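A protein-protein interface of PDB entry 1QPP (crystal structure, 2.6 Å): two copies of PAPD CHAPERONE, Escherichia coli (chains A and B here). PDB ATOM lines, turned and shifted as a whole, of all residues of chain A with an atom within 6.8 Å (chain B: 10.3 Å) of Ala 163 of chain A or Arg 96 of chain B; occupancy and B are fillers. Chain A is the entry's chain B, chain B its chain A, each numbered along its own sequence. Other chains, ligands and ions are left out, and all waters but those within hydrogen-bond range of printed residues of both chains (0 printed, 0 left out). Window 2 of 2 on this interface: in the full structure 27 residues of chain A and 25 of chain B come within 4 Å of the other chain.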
ATOM      1  N   VAL A 153      16.044 -19.666  -1.182  1.00  0.00           N
ATOM      2  CA  VAL A 153      14.953 -20.353  -1.885  1.00  0.00           C
ATOM      3  C   VAL A 153      14.553 -19.503  -3.084  1.00  0.00           C
ATOM      4  O   VAL A 153      14.157 -18.350  -2.882  1.00  0.00           O
ATOM      5  CB  VAL A 153      13.754 -20.620  -0.964  1.00  0.00           C
ATOM      6  CG1 VAL A 153      12.543 -21.103  -1.730  1.00  0.00           C
ATOM      7  CG2 VAL A 153      14.216 -21.675   0.047  1.00  0.00           C
ATOM      8  N   ILE A 154      14.702 -20.053  -4.290  1.00  0.00           N
ATOM      9  CA  ILE A 154      14.386 -19.296  -5.500  1.00  0.00           C
ATOM     10  C   ILE A 154      13.102 -19.735  -6.187  1.00  0.00           C
ATOM     11  O   ILE A 154      12.626 -19.097  -7.140  1.00  0.00           O
ATOM     12  CB  ILE A 154      15.546 -19.359  -6.514  1.00  0.00           C
ATOM     13  CG1 ILE A 154      15.917 -20.809  -6.795  1.00  0.00           C
ATOM     14  CG2 ILE A 154      16.731 -18.588  -5.946  1.00  0.00           C
ATOM     15  CD1 ILE A 154      16.864 -21.007  -7.952  1.00  0.00           C
ATOM     16  N   GLY A 155      12.468 -20.812  -5.716  1.00  0.00           N
ATOM     17  CA  GLY A 155      11.210 -21.259  -6.287  1.00  0.00           C
ATOM     18  C   GLY A 155      10.433 -22.281  -5.477  1.00  0.00           C
ATOM     19  O   GLY A 155      10.980 -23.213  -4.879  1.00  0.00           O
ATOM     20  N   LEU A 156       9.113 -22.116  -5.506  1.00  0.00           N
ATOM     21  CA  LEU A 156       8.233 -23.069  -4.809  1.00  0.00           C
ATOM     22  C   LEU A 156       7.043 -23.381  -5.703  1.00  0.00           C
ATOM     23  O   LEU A 156       6.405 -22.464  -6.212  1.00  0.00           O
ATOM     24  CB  LEU A 156       7.851 -22.511  -3.452  1.00  0.00           C
ATOM     25  CG  LEU A 156       6.793 -23.232  -2.635  1.00  0.00           C
ATOM     26  CD1 LEU A 156       7.227 -24.620  -2.199  1.00  0.00           C
ATOM     27  CD2 LEU A 156       6.457 -22.375  -1.416  1.00  0.00           C
ATOM     28  N   GLY A 157       6.799 -24.654  -5.992  1.00  0.00           N
ATOM     29  CA  GLY A 157       5.708 -25.023  -6.882  1.00  0.00           C
ATOM     30  C   GLY A 157       5.050 -26.381  -6.682  1.00  0.00           C
ATOM     31  O   GLY A 157       5.297 -27.145  -5.739  1.00  0.00           O
ATOM     32  N   GLY A 158       4.136 -26.688  -7.615  1.00  0.00           N
ATOM     33  CA  GLY A 158       3.412 -27.951  -7.620  1.00  0.00           C
ATOM     34  C   GLY A 158       4.201 -29.051  -8.309  1.00  0.00           C
ATOM     35  O   GLY A 158       4.039 -30.214  -7.955  1.00  0.00           O
ATOM     36  N   SER A 159       5.094 -28.706  -9.221  1.00  0.00           N
ATOM     37  CA  SER A 159       5.899 -29.736  -9.881  1.00  0.00           C
ATOM     38  C   SER A 159       7.349 -29.299 -10.018  1.00  0.00           C
ATOM     39  O   SER A 159       7.718 -28.147  -9.777  1.00  0.00           O
ATOM     40  CB  SER A 159       5.277 -29.995 -11.257  1.00  0.00           C
ATOM     41  OG  SER A 159       5.271 -28.742 -11.939  1.00  0.00           O
ATOM     42  N   GLU A 160       8.200 -30.221 -10.446  1.00  0.00           N
ATOM     43  CA  GLU A 160       9.619 -29.936 -10.644  1.00  0.00           C
ATOM     44  C   GLU A 160       9.812 -28.745 -11.575  1.00  0.00           C
ATOM     45  O   GLU A 160      10.653 -27.887 -11.312  1.00  0.00           O
ATOM     46  CB  GLU A 160      10.329 -31.190 -11.146  1.00  0.00           C
ATOM     47  CG  GLU A 160      11.835 -31.099 -11.228  1.00  0.00           C
ATOM     48  CD  GLU A 160      12.496 -32.341 -11.803  1.00  0.00           C
ATOM     49  OE1 GLU A 160      13.496 -32.842 -11.230  1.00  0.00           O
ATOM     50  OE2 GLU A 160      12.017 -32.820 -12.852  1.00  0.00           O
ATOM     51  N   LYS A 161       9.019 -28.647 -12.631  1.00  0.00           N
ATOM     52  CA  LYS A 161       9.086 -27.554 -13.582  1.00  0.00           C
ATOM     53  C   LYS A 161       8.442 -26.278 -13.054  1.00  0.00           C
ATOM     54  O   LYS A 161       8.954 -25.185 -13.337  1.00  0.00           O
ATOM     55  CB  LYS A 161       8.443 -27.943 -14.920  1.00  0.00           C
ATOM     56  CG  LYS A 161       9.235 -28.960 -15.715  1.00  0.00           C
ATOM     57  CD  LYS A 161      10.089 -28.275 -16.775  1.00  0.00           C
ATOM     58  CE  LYS A 161      11.106 -29.227 -17.379  1.00  0.00           C
ATOM     59  NZ  LYS A 161      12.488 -28.687 -17.523  1.00  0.00           N
ATOM     60  N   GLN A 162       7.376 -26.393 -12.248  1.00  0.00           N
ATOM     61  CA  GLN A 162       6.754 -25.189 -11.694  1.00  0.00           C
ATOM     62  C   GLN A 162       7.665 -24.613 -10.615  1.00  0.00           C
ATOM     63  O   GLN A 162       7.575 -23.433 -10.298  1.00  0.00           O
ATOM     64  CB  GLN A 162       5.331 -25.396 -11.209  1.00  0.00           C
ATOM     65  N   ALA A 163       8.599 -25.394 -10.097  1.00  0.00           N
ATOM     66  CA  ALA A 163       9.610 -24.978  -9.148  1.00  0.00           C
ATOM     67  C   ALA A 163      10.778 -24.277  -9.854  1.00  0.00           C
ATOM     68  O   ALA A 163      11.566 -23.627  -9.163  1.00  0.00           O
ATOM     69  CB  ALA A 163      10.187 -26.141  -8.348  1.00  0.00           C
ATOM     70  N   GLU A 164      10.906 -24.425 -11.169  1.00  0.00           N
ATOM     71  CA  GLU A 164      11.963 -23.750 -11.902  1.00  0.00           C
ATOM     72  C   GLU A 164      11.341 -22.664 -12.774  1.00  0.00           C
ATOM     73  O   GLU A 164      12.076 -22.037 -13.515  1.00  0.00           O
ATOM     74  CB  GLU A 164      12.822 -24.659 -12.764  1.00  0.00           C
ATOM     75  CG  GLU A 164      13.294 -25.925 -12.078  1.00  0.00           C
ATOM     76  CD  GLU A 164      13.695 -27.017 -13.045  1.00  0.00           C
ATOM     77  OE1 GLU A 164      13.939 -26.729 -14.239  1.00  0.00           O
ATOM     78  OE2 GLU A 164      13.780 -28.185 -12.609  1.00  0.00           O
ATOM     79  N   GLU A 165      10.045 -22.452 -12.633  1.00  0.00           N
ATOM     80  CA  GLU A 165       9.343 -21.424 -13.391  1.00  0.00           C
ATOM     81  C   GLU A 165       9.387 -20.090 -12.657  1.00  0.00           C
ATOM     82  O   GLU A 165       8.939 -19.075 -13.191  1.00  0.00           O
ATOM     83  CB  GLU A 165       7.893 -21.846 -13.653  1.00  0.00           C
ATOM     84  N   GLY A 166       9.892 -20.074 -11.431  1.00  0.00           N
ATOM     85  CA  GLY A 166      10.001 -18.874 -10.619  1.00  0.00           C
ATOM     86  C   GLY A 166      10.967 -17.898 -11.291  1.00  0.00           C
ATOM     87  O   GLY A 166      12.019 -18.290 -11.802  1.00  0.00           O
ATOM     88  N   GLU A 167      10.578 -16.628 -11.293  1.00  0.00           N
ATOM     89  CA  GLU A 167      11.365 -15.570 -11.906  1.00  0.00           C
ATOM     90  C   GLU A 167      12.150 -14.759 -10.880  1.00  0.00           C
ATOM     91  O   GLU A 167      13.379 -14.711 -10.930  1.00  0.00           O
ATOM     92  CB  GLU A 167      10.446 -14.625 -12.695  1.00  0.00           C
ATOM     93  CG  GLU A 167       9.800 -15.233 -13.925  1.00  0.00           C
ATOM     94  CD  GLU A 167       8.905 -14.256 -14.663  1.00  0.00           C
ATOM     95  OE1 GLU A 167       8.988 -14.211 -15.911  1.00  0.00           O
ATOM     96  OE2 GLU A 167       8.120 -13.533 -14.011  1.00  0.00           O
ATOM     97  N   PHE A 168      11.418 -14.051 -10.015  1.00  0.00           N
ATOM     98  CA  PHE A 168      12.015 -13.167  -9.030  1.00  0.00           C
ATOM     99  C   PHE A 168      11.530 -13.405  -7.605  1.00  0.00           C
ATOM    100  O   PHE A 168      11.552 -12.487  -6.769  1.00  0.00           O
ATOM    101  CB  PHE A 168      11.710 -11.707  -9.411  1.00  0.00           C
ATOM    102  CG  PHE A 168      11.935 -11.303 -10.836  1.00  0.00           C
ATOM    103  CD1 PHE A 168      13.208 -11.155 -11.350  1.00  0.00           C
ATOM    104  CD2 PHE A 168      10.849 -11.101 -11.671  1.00  0.00           C
ATOM    105  CE1 PHE A 168      13.385 -10.791 -12.664  1.00  0.00           C
ATOM    106  CE2 PHE A 168      11.020 -10.726 -12.989  1.00  0.00           C
ATOM    107  CZ  PHE A 168      12.298 -10.579 -13.490  1.00  0.00           C
ATOM    108  N   GLU A 169      11.138 -14.628  -7.256  1.00  0.00           N
ATOM    109  CA  GLU A 169      10.623 -14.884  -5.909  1.00  0.00           C
ATOM    110  C   GLU A 169      11.644 -15.401  -4.912  1.00  0.00           C
ATOM    111  O   GLU A 169      11.336 -16.213  -4.025  1.00  0.00           O
ATOM    112  CB  GLU A 169       9.371 -15.755  -6.056  1.00  0.00           C
ATOM    113  CG  GLU A 169       9.567 -17.247  -6.190  1.00  0.00           C
ATOM    114  CD  GLU A 169       8.930 -18.025  -5.045  1.00  0.00           C
ATOM    115  OE1 GLU A 169       9.610 -18.455  -4.082  1.00  0.00           O
ATOM    116  OE2 GLU A 169       7.692 -18.222  -5.111  1.00  0.00           O
ATOM    117  N   THR A 170      12.871 -14.885  -4.890  1.00  0.00           N
ATOM    118  CA  THR A 170      13.897 -15.295  -3.947  1.00  0.00           C
ATOM    119  C   THR A 170      13.563 -14.982  -2.489  1.00  0.00           C
ATOM    120  O   THR A 170      13.113 -13.900  -2.127  1.00  0.00           O
ATOM    121  CB  THR A 170      15.274 -14.719  -4.299  1.00  0.00           C
ATOM    122  OG1 THR A 170      15.804 -15.394  -5.439  1.00  0.00           O
ATOM    123  CG2 THR A 170      16.314 -14.912  -3.206  1.00  0.00           C
ATOM    124  N   TYR A 190       7.264 -28.694  -4.379  1.00  0.00           N
ATOM    125  CA  TYR A 190       8.643 -28.809  -4.834  1.00  0.00           C
ATOM    126  C   TYR A 190       9.306 -27.459  -4.537  1.00  0.00           C
ATOM    127  O   TYR A 190       8.637 -26.425  -4.642  1.00  0.00           O
ATOM    128  CB  TYR A 190       8.755 -29.115  -6.310  1.00  0.00           C
ATOM    129  CG  TYR A 190       8.327 -30.498  -6.729  1.00  0.00           C
ATOM    130  CD1 TYR A 190       6.996 -30.897  -6.734  1.00  0.00           C
ATOM    131  CD2 TYR A 190       9.290 -31.405  -7.153  1.00  0.00           C
ATOM    132  CE1 TYR A 190       6.640 -32.162  -7.146  1.00  0.00           C
ATOM    133  CE2 TYR A 190       8.936 -32.673  -7.567  1.00  0.00           C
ATOM    134  CZ  TYR A 190       7.608 -33.045  -7.569  1.00  0.00           C
ATOM    135  OH  TYR A 190       7.291 -34.324  -7.982  1.00  0.00           O
ATOM    136  N   LEU A 191      10.572 -27.534  -4.154  1.00  0.00           N
ATOM    137  CA  LEU A 191      11.265 -26.299  -3.771  1.00  0.00           C
ATOM    138  C   LEU A 191      12.628 -26.236  -4.435  1.00  0.00           C
ATOM    139  O   LEU A 191      13.354 -27.241  -4.394  1.00  0.00           O
ATOM    140  CB  LEU A 191      11.362 -26.301  -2.246  1.00  0.00           C
ATOM    141  CG  LEU A 191      11.945 -25.111  -1.511  1.00  0.00           C
ATOM    142  CD1 LEU A 191      11.419 -25.061  -0.083  1.00  0.00           C
ATOM    143  CD2 LEU A 191      13.465 -25.144  -1.527  1.00  0.00           C
ATOM    144  N   SER A 192      12.949 -25.059  -4.976  1.00  0.00           N
ATOM    145  CA  SER A 192      14.260 -24.949  -5.633  1.00  0.00           C
ATOM    146  C   SER A 192      15.146 -24.001  -4.835  1.00  0.00           C
ATOM    147  O   SER A 192      14.661 -22.982  -4.344  1.00  0.00           O
ATOM    148  CB  SER A 192      14.088 -24.498  -7.079  1.00  0.00           C
ATOM    149  OG  SER A 192      15.322 -24.488  -7.744  1.00  0.00           O
ATOM    150  N   TYR A 193      16.423 -24.325  -4.710  1.00  0.00           N
ATOM    151  CA  TYR A 193      17.346 -23.518  -3.929  1.00  0.00           C
ATOM    152  C   TYR A 193      18.695 -23.393  -4.629  1.00  0.00           C
ATOM    153  O   TYR A 193      19.006 -24.228  -5.459  1.00  0.00           O
ATOM    154  CB  TYR A 193      17.611 -24.141  -2.545  1.00  0.00           C
ATOM    155  CG  TYR A 193      18.297 -25.489  -2.586  1.00  0.00           C
ATOM    156  CD1 TYR A 193      17.562 -26.657  -2.763  1.00  0.00           C
ATOM    157  CD2 TYR A 193      19.676 -25.594  -2.463  1.00  0.00           C
ATOM    158  CE1 TYR A 193      18.177 -27.888  -2.812  1.00  0.00           C
ATOM    159  CE2 TYR A 193      20.305 -26.823  -2.514  1.00  0.00           C
ATOM    160  CZ  TYR A 193      19.548 -27.971  -2.678  1.00  0.00           C
ATOM    161  OH  TYR A 193      20.220 -29.177  -2.734  1.00  0.00           O
ATOM    162  N   ARG A 200      21.223 -25.086  -9.017  1.00  0.00           N
ATOM    163  CA  ARG A 200      19.839 -24.896  -8.654  1.00  0.00           C
ATOM    164  C   ARG A 200      19.090 -26.212  -8.555  1.00  0.00           C
ATOM    165  O   ARG A 200      18.224 -26.487  -9.378  1.00  0.00           O
ATOM    166  CB  ARG A 200      19.143 -24.023  -9.723  1.00  0.00           C
ATOM    167  CG  ARG A 200      19.614 -22.597  -9.869  1.00  0.00           C
ATOM    168  CD  ARG A 200      19.322 -21.989 -11.225  1.00  0.00           C
ATOM    169  NE  ARG A 200      20.177 -20.849 -11.547  1.00  0.00           N
ATOM    170  CZ  ARG A 200      20.074 -19.626 -11.037  1.00  0.00           C
ATOM    171  NH1 ARG A 200      20.911 -18.655 -11.398  1.00  0.00           N
ATOM    172  NH2 ARG A 200      19.130 -19.335 -10.148  1.00  0.00           N
ATOM    173  N   PRO A 201      19.377 -27.038  -7.577  1.00  0.00           N
ATOM    174  CA  PRO A 201      18.674 -28.284  -7.322  1.00  0.00           C
ATOM    175  C   PRO A 201      17.202 -28.037  -6.998  1.00  0.00           C
ATOM    176  O   PRO A 201      16.794 -26.899  -6.758  1.00  0.00           O
ATOM    177  CB  PRO A 201      19.327 -28.955  -6.091  1.00  0.00           C
ATOM    178  CG  PRO A 201      20.498 -28.062  -5.800  1.00  0.00           C
ATOM    179  CD  PRO A 201      20.376 -26.762  -6.543  1.00  0.00           C
ATOM    180  N   VAL A 202      16.408 -29.101  -6.996  1.00  0.00           N
ATOM    181  CA  VAL A 202      15.002 -29.039  -6.626  1.00  0.00           C
ATOM    182  C   VAL A 202      14.795 -30.189  -5.632  1.00  0.00           C
ATOM    183  O   VAL A 202      15.480 -31.209  -5.728  1.00  0.00           O
ATOM    184  CB  VAL A 202      13.991 -29.129  -7.763  1.00  0.00           C
ATOM    185  CG1 VAL A 202      12.586 -29.403  -7.240  1.00  0.00           C
ATOM    186  CG2 VAL A 202      13.948 -27.828  -8.562  1.00  0.00           C
ATOM    187  N   LEU A 203      13.910 -29.979  -4.674  1.00  0.00           N
ATOM    188  CA  LEU A 203      13.582 -30.969  -3.668  1.00  0.00           C
ATOM    189  C   LEU A 203      12.113 -31.375  -3.752  1.00  0.00           C
ATOM    190  O   LEU A 203      11.244 -30.624  -4.210  1.00  0.00           O
ATOM    191  CB  LEU A 203      13.900 -30.388  -2.286  1.00  0.00           C
ATOM    192  CG  LEU A 203      15.370 -30.033  -2.043  1.00  0.00           C
ATOM    193  CD1 LEU A 203      15.582 -29.462  -0.655  1.00  0.00           C
ATOM    194  CD2 LEU A 203      16.264 -31.237  -2.295  1.00  0.00           C
ATOM    195  N   LEU B  29      13.506 -11.903 -22.235  1.00  0.00           N
ATOM    196  CA  LEU B  29      13.220 -11.976 -20.797  1.00  0.00           C
ATOM    197  C   LEU B  29      12.930 -10.621 -20.164  1.00  0.00           C
ATOM    198  O   LEU B  29      13.487  -9.598 -20.561  1.00  0.00           O
ATOM    199  CB  LEU B  29      14.457 -12.576 -20.091  1.00  0.00           C
ATOM    200  CG  LEU B  29      14.753 -14.043 -20.390  1.00  0.00           C
ATOM    201  CD1 LEU B  29      16.203 -14.360 -20.096  1.00  0.00           C
ATOM    202  CD2 LEU B  29      13.783 -14.958 -19.660  1.00  0.00           C
ATOM    203  N   PRO B  30      12.105 -10.578 -19.136  1.00  0.00           N
ATOM    204  CA  PRO B  30      11.751  -9.396 -18.355  1.00  0.00           C
ATOM    205  C   PRO B  30      12.700  -9.136 -17.188  1.00  0.00           C
ATOM    206  O   PRO B  30      13.485  -9.991 -16.758  1.00  0.00           O
ATOM    207  CB  PRO B  30      10.313  -9.646 -17.864  1.00  0.00           C
ATOM    208  CG  PRO B  30      10.286 -11.140 -17.789  1.00  0.00           C
ATOM    209  CD  PRO B  30      11.388 -11.758 -18.621  1.00  0.00           C
ATOM    210  N   TYR B  31      12.766  -7.896 -16.719  1.00  0.00           N
ATOM    211  CA  TYR B  31      13.715  -7.470 -15.706  1.00  0.00           C
ATOM    212  C   TYR B  31      12.995  -6.633 -14.652  1.00  0.00           C
ATOM    213  O   TYR B  31      12.002  -6.009 -15.002  1.00  0.00           O
ATOM    214  CB  TYR B  31      14.833  -6.585 -16.303  1.00  0.00           C
ATOM    215  CG  TYR B  31      16.022  -7.382 -16.775  1.00  0.00           C
ATOM    216  CD1 TYR B  31      15.937  -8.087 -17.968  1.00  0.00           C
ATOM    217  CD2 TYR B  31      17.214  -7.441 -16.065  1.00  0.00           C
ATOM    218  CE1 TYR B  31      16.989  -8.841 -18.438  1.00  0.00           C
ATOM    219  CE2 TYR B  31      18.269  -8.198 -16.520  1.00  0.00           C
ATOM    220  CZ  TYR B  31      18.160  -8.891 -17.708  1.00  0.00           C
ATOM    221  OH  TYR B  31      19.204  -9.644 -18.203  1.00  0.00           O
ATOM    222  N   LEU B  32      13.541  -6.674 -13.442  1.00  0.00           N
ATOM    223  CA  LEU B  32      13.055  -5.832 -12.356  1.00  0.00           C
ATOM    224  C   LEU B  32      13.943  -4.576 -12.373  1.00  0.00           C
ATOM    225  O   LEU B  32      15.040  -4.596 -12.933  1.00  0.00           O
ATOM    226  CB  LEU B  32      13.164  -6.500 -11.007  1.00  0.00           C
ATOM    227  CG  LEU B  32      12.169  -7.568 -10.562  1.00  0.00           C
ATOM    228  CD1 LEU B  32      12.522  -7.966  -9.123  1.00  0.00           C
ATOM    229  CD2 LEU B  32      10.716  -7.147 -10.632  1.00  0.00           C
ATOM    230  N   ARG B  58       8.282  -3.942 -12.557  1.00  0.00           N
ATOM    231  CA  ARG B  58       8.574  -5.032 -13.510  1.00  0.00           C
ATOM    232  C   ARG B  58       8.563  -4.402 -14.905  1.00  0.00           C
ATOM    233  O   ARG B  58       7.770  -3.501 -15.208  1.00  0.00           O
ATOM    234  CB  ARG B  58       7.573  -6.173 -13.335  1.00  0.00           C
ATOM    235  CG  ARG B  58       7.821  -7.453 -14.075  1.00  0.00           C
ATOM    236  CD  ARG B  58       6.557  -8.272 -14.366  1.00  0.00           C
ATOM    237  NE  ARG B  58       6.982  -9.658 -14.614  1.00  0.00           N
ATOM    238  CZ  ARG B  58       6.958 -10.290 -15.772  1.00  0.00           C
ATOM    239  NH1 ARG B  58       7.395 -11.542 -15.843  1.00  0.00           N
ATOM    240  NH2 ARG B  58       6.502  -9.690 -16.869  1.00  0.00           N
ATOM    241  N   ILE B  93      17.292  -6.304 -11.786  1.00  0.00           N
ATOM    242  CA  ILE B  93      17.314  -7.671 -11.269  1.00  0.00           C
ATOM    243  C   ILE B  93      16.887  -8.611 -12.383  1.00  0.00           C
ATOM    244  O   ILE B  93      15.764  -8.620 -12.879  1.00  0.00           O
ATOM    245  CB  ILE B  93      16.415  -7.794 -10.022  1.00  0.00           C
ATOM    246  CG1 ILE B  93      16.871  -6.785  -8.962  1.00  0.00           C
ATOM    247  CG2 ILE B  93      16.468  -9.194  -9.415  1.00  0.00           C
ATOM    248  CD1 ILE B  93      16.400  -5.365  -9.149  1.00  0.00           C
ATOM    249  N   PRO B  94      17.804  -9.432 -12.839  1.00  0.00           N
ATOM    250  CA  PRO B  94      17.584 -10.393 -13.908  1.00  0.00           C
ATOM    251  C   PRO B  94      16.719 -11.554 -13.464  1.00  0.00           C
ATOM    252  O   PRO B  94      16.656 -11.886 -12.286  1.00  0.00           O
ATOM    253  CB  PRO B  94      18.988 -10.898 -14.309  1.00  0.00           C
ATOM    254  CG  PRO B  94      19.795 -10.625 -13.071  1.00  0.00           C
ATOM    255  CD  PRO B  94      19.170  -9.491 -12.297  1.00  0.00           C
ATOM    256  N   PRO B  95      15.975 -12.158 -14.366  1.00  0.00           N
ATOM    257  CA  PRO B  95      15.083 -13.275 -14.088  1.00  0.00           C
ATOM    258  C   PRO B  95      15.862 -14.576 -14.058  1.00  0.00           C
ATOM    259  O   PRO B  95      16.967 -14.601 -14.593  1.00  0.00           O
ATOM    260  CB  PRO B  95      14.027 -13.261 -15.215  1.00  0.00           C
ATOM    261  CG  PRO B  95      14.794 -12.607 -16.335  1.00  0.00           C
ATOM    262  CD  PRO B  95      15.940 -11.777 -15.790  1.00  0.00           C
ATOM    263  N   ARG B  96      15.331 -15.639 -13.469  1.00  0.00           N
ATOM    264  CA  ARG B  96      16.049 -16.912 -13.434  1.00  0.00           C
ATOM    265  C   ARG B  96      15.861 -17.744 -14.692  1.00  0.00           C
ATOM    266  O   ARG B  96      14.816 -18.212 -15.112  1.00  0.00           O
ATOM    267  CB  ARG B  96      15.652 -17.702 -12.187  1.00  0.00           C
ATOM    268  CG  ARG B  96      16.266 -19.093 -12.114  1.00  0.00           C
ATOM    269  CD  ARG B  96      15.248 -20.152 -12.491  1.00  0.00           C
ATOM    270  NE  ARG B  96      14.657 -20.855 -11.371  1.00  0.00           N
ATOM    271  CZ  ARG B  96      14.047 -20.358 -10.308  1.00  0.00           C
ATOM    272  NH1 ARG B  96      13.907 -19.055 -10.125  1.00  0.00           N
ATOM    273  NH2 ARG B  96      13.558 -21.181  -9.384  1.00  0.00           N
ATOM    274  N   GLN B 104      24.545 -14.578 -14.317  1.00  0.00           N
ATOM    275  CA  GLN B 104      23.294 -14.130 -13.739  1.00  0.00           C
ATOM    276  C   GLN B 104      23.375 -13.405 -12.399  1.00  0.00           C
ATOM    277  O   GLN B 104      23.031 -13.942 -11.340  1.00  0.00           O
ATOM    278  CB  GLN B 104      22.331 -15.314 -13.539  1.00  0.00           C
ATOM    279  CG  GLN B 104      20.931 -14.799 -13.187  1.00  0.00           C
ATOM    280  CD  GLN B 104      19.935 -15.925 -13.002  1.00  0.00           C
ATOM    281  OE1 GLN B 104      19.743 -16.699 -13.940  1.00  0.00           O
ATOM    282  NE2 GLN B 104      19.329 -16.008 -11.825  1.00  0.00           N
ATOM    283  N   ILE B 105      23.775 -12.133 -12.417  1.00  0.00           N
ATOM    284  CA  ILE B 105      23.882 -11.283 -11.246  1.00  0.00           C
ATOM    285  C   ILE B 105      23.315  -9.888 -11.537  1.00  0.00           C
ATOM    286  O   ILE B 105      23.390  -9.406 -12.662  1.00  0.00           O
ATOM    287  CB  ILE B 105      25.343 -11.111 -10.780  1.00  0.00           C
ATOM    288  CG1 ILE B 105      26.283 -10.918 -11.977  1.00  0.00           C
ATOM    289  CG2 ILE B 105      25.790 -12.313  -9.964  1.00  0.00           C
ATOM    290  CD1 ILE B 105      27.680 -10.474 -11.618  1.00  0.00           C
ATOM    291  N   ALA B 106      22.748  -9.272 -10.515  1.00  0.00           N
ATOM    292  CA  ALA B 106      22.187  -7.946 -10.557  1.00  0.00           C
ATOM    293  C   ALA B 106      23.244  -6.882 -10.822  1.00  0.00           C
ATOM    294  O   ALA B 106      24.339  -6.965 -10.276  1.00  0.00           O
ATOM    295  CB  ALA B 106      21.560  -7.617  -9.196  1.00  0.00           C
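Among the printed residues, merely in contact across the chains: Phe 168 of chain A with Ile 93 of chain B (3.2 Å), Phe 168 of chain A with Pro 95 of chain B (3.3 Å), Phe 168 of chain A with Pro 94 of chain B (3.5 Å), Arg 200 of chain A with Arg 96 of chain B (3.5 Å), Phe 168 of chain A with Pro 30 of chain B (3.5 Å), Glu 164 of chain A with Arg 96 of chain B (3.6 Å), Phe 168 of chain A with Leu 32 of chain B (3.8 Å), Glu 167 of chain A with Pro 30 of chain B (3.8 Å), Gly 155 of chain A with Arg 96 of chain B (3.8 Å) and Glu 167 of chain A with Pro 95 of chain B (3.9 Å).
NH1 of Arg 58 of chain B is in salt-bridge range of OE2 of Glu 167 of chain A, 2.8 Å away. The guanidinium group of Arg 96 of chain B is in hydrogen-bond range of the backbone carbonyl oxygen of Ile 154 of chain A (3.2 Å). The backbone carbonyl oxygen (O) of Ala 163 of chain A sits at hydrogen-bond distance from the guanidinium group (NH2) of Arg 96 of chain B. The guanidinium group (NH1) of Arg 96 of chain B lies within hydrogen-bond range of the backbone carbonyl oxygen (O) of Gly 166 of chain A, 2.6 Å away. O of Glu 167 of chain A lies within hydrogen-bond range of N of Arg 96 of chain B, 3.3 Å away. The side-chain amide nitrogen of Gln 104 of chain B lies close to the guanidinium group of Arg 200 of chain A.
Of the 26 printed residues of chain A, 8 touch a printed residue of chain B. Hydrophobic or aromatic side chains of chain A that line the printed part of chain B: Ile 154 and Phe 168. Among the printed residues, Asp or Glu carboxylates within 4 Å of a Lys or Arg side-chain nitrogen of the other chain: Glu 167 of chain A with Arg 58 of chain B (2.8 Å).
No position is printed for both chains.
Ile 154 of chain A touches one residue of chain B. Gly 155 of chain A touches just one residue of chain B: Arg 96. No residue of chain B comes within 4 Å of Gly 157 of chain A. No residue of chain B comes within 4 Å of Ser 159 of chain A. No residue of chain B comes within 4 Å of Gln 162 of chain A. Ala 163 of chain A touches just one residue of chain B: Arg 96 (3.2 Å). Of the printed residues of chain B, Glu 164 of chain A touches Arg 96. Printed residues of chain A within 4 Å of Pro 30 of chain B: Glu 167 and Phe 168. Of the printed residues of chain A, Gln 104 of chain B touches Arg 200. The nearest printed residue of chain B that does not touch Ala 163 of chain A is Pro 95 of chain B (11.2 Å). The nearest printed residue of chain B that does not touch Phe 168 of chain A is Tyr 31 of chain B (4.1 Å).
The backbone NH (N) of Leu 32 of chain B is in hydrogen-bond range of the backbone carbonyl oxygen (O) of Ile 93 of chain B (3.0 Å). N of Ile 154 of chain A sits at hydrogen-bond distance from O of Ser 192 of chain A, 2.9 Å away. The backbone carbonyl oxygen (O) of Gly 155 of chain A sits at hydrogen-bond distance from the backbone NH (N) of Ser 192 of chain A (2.7 Å).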
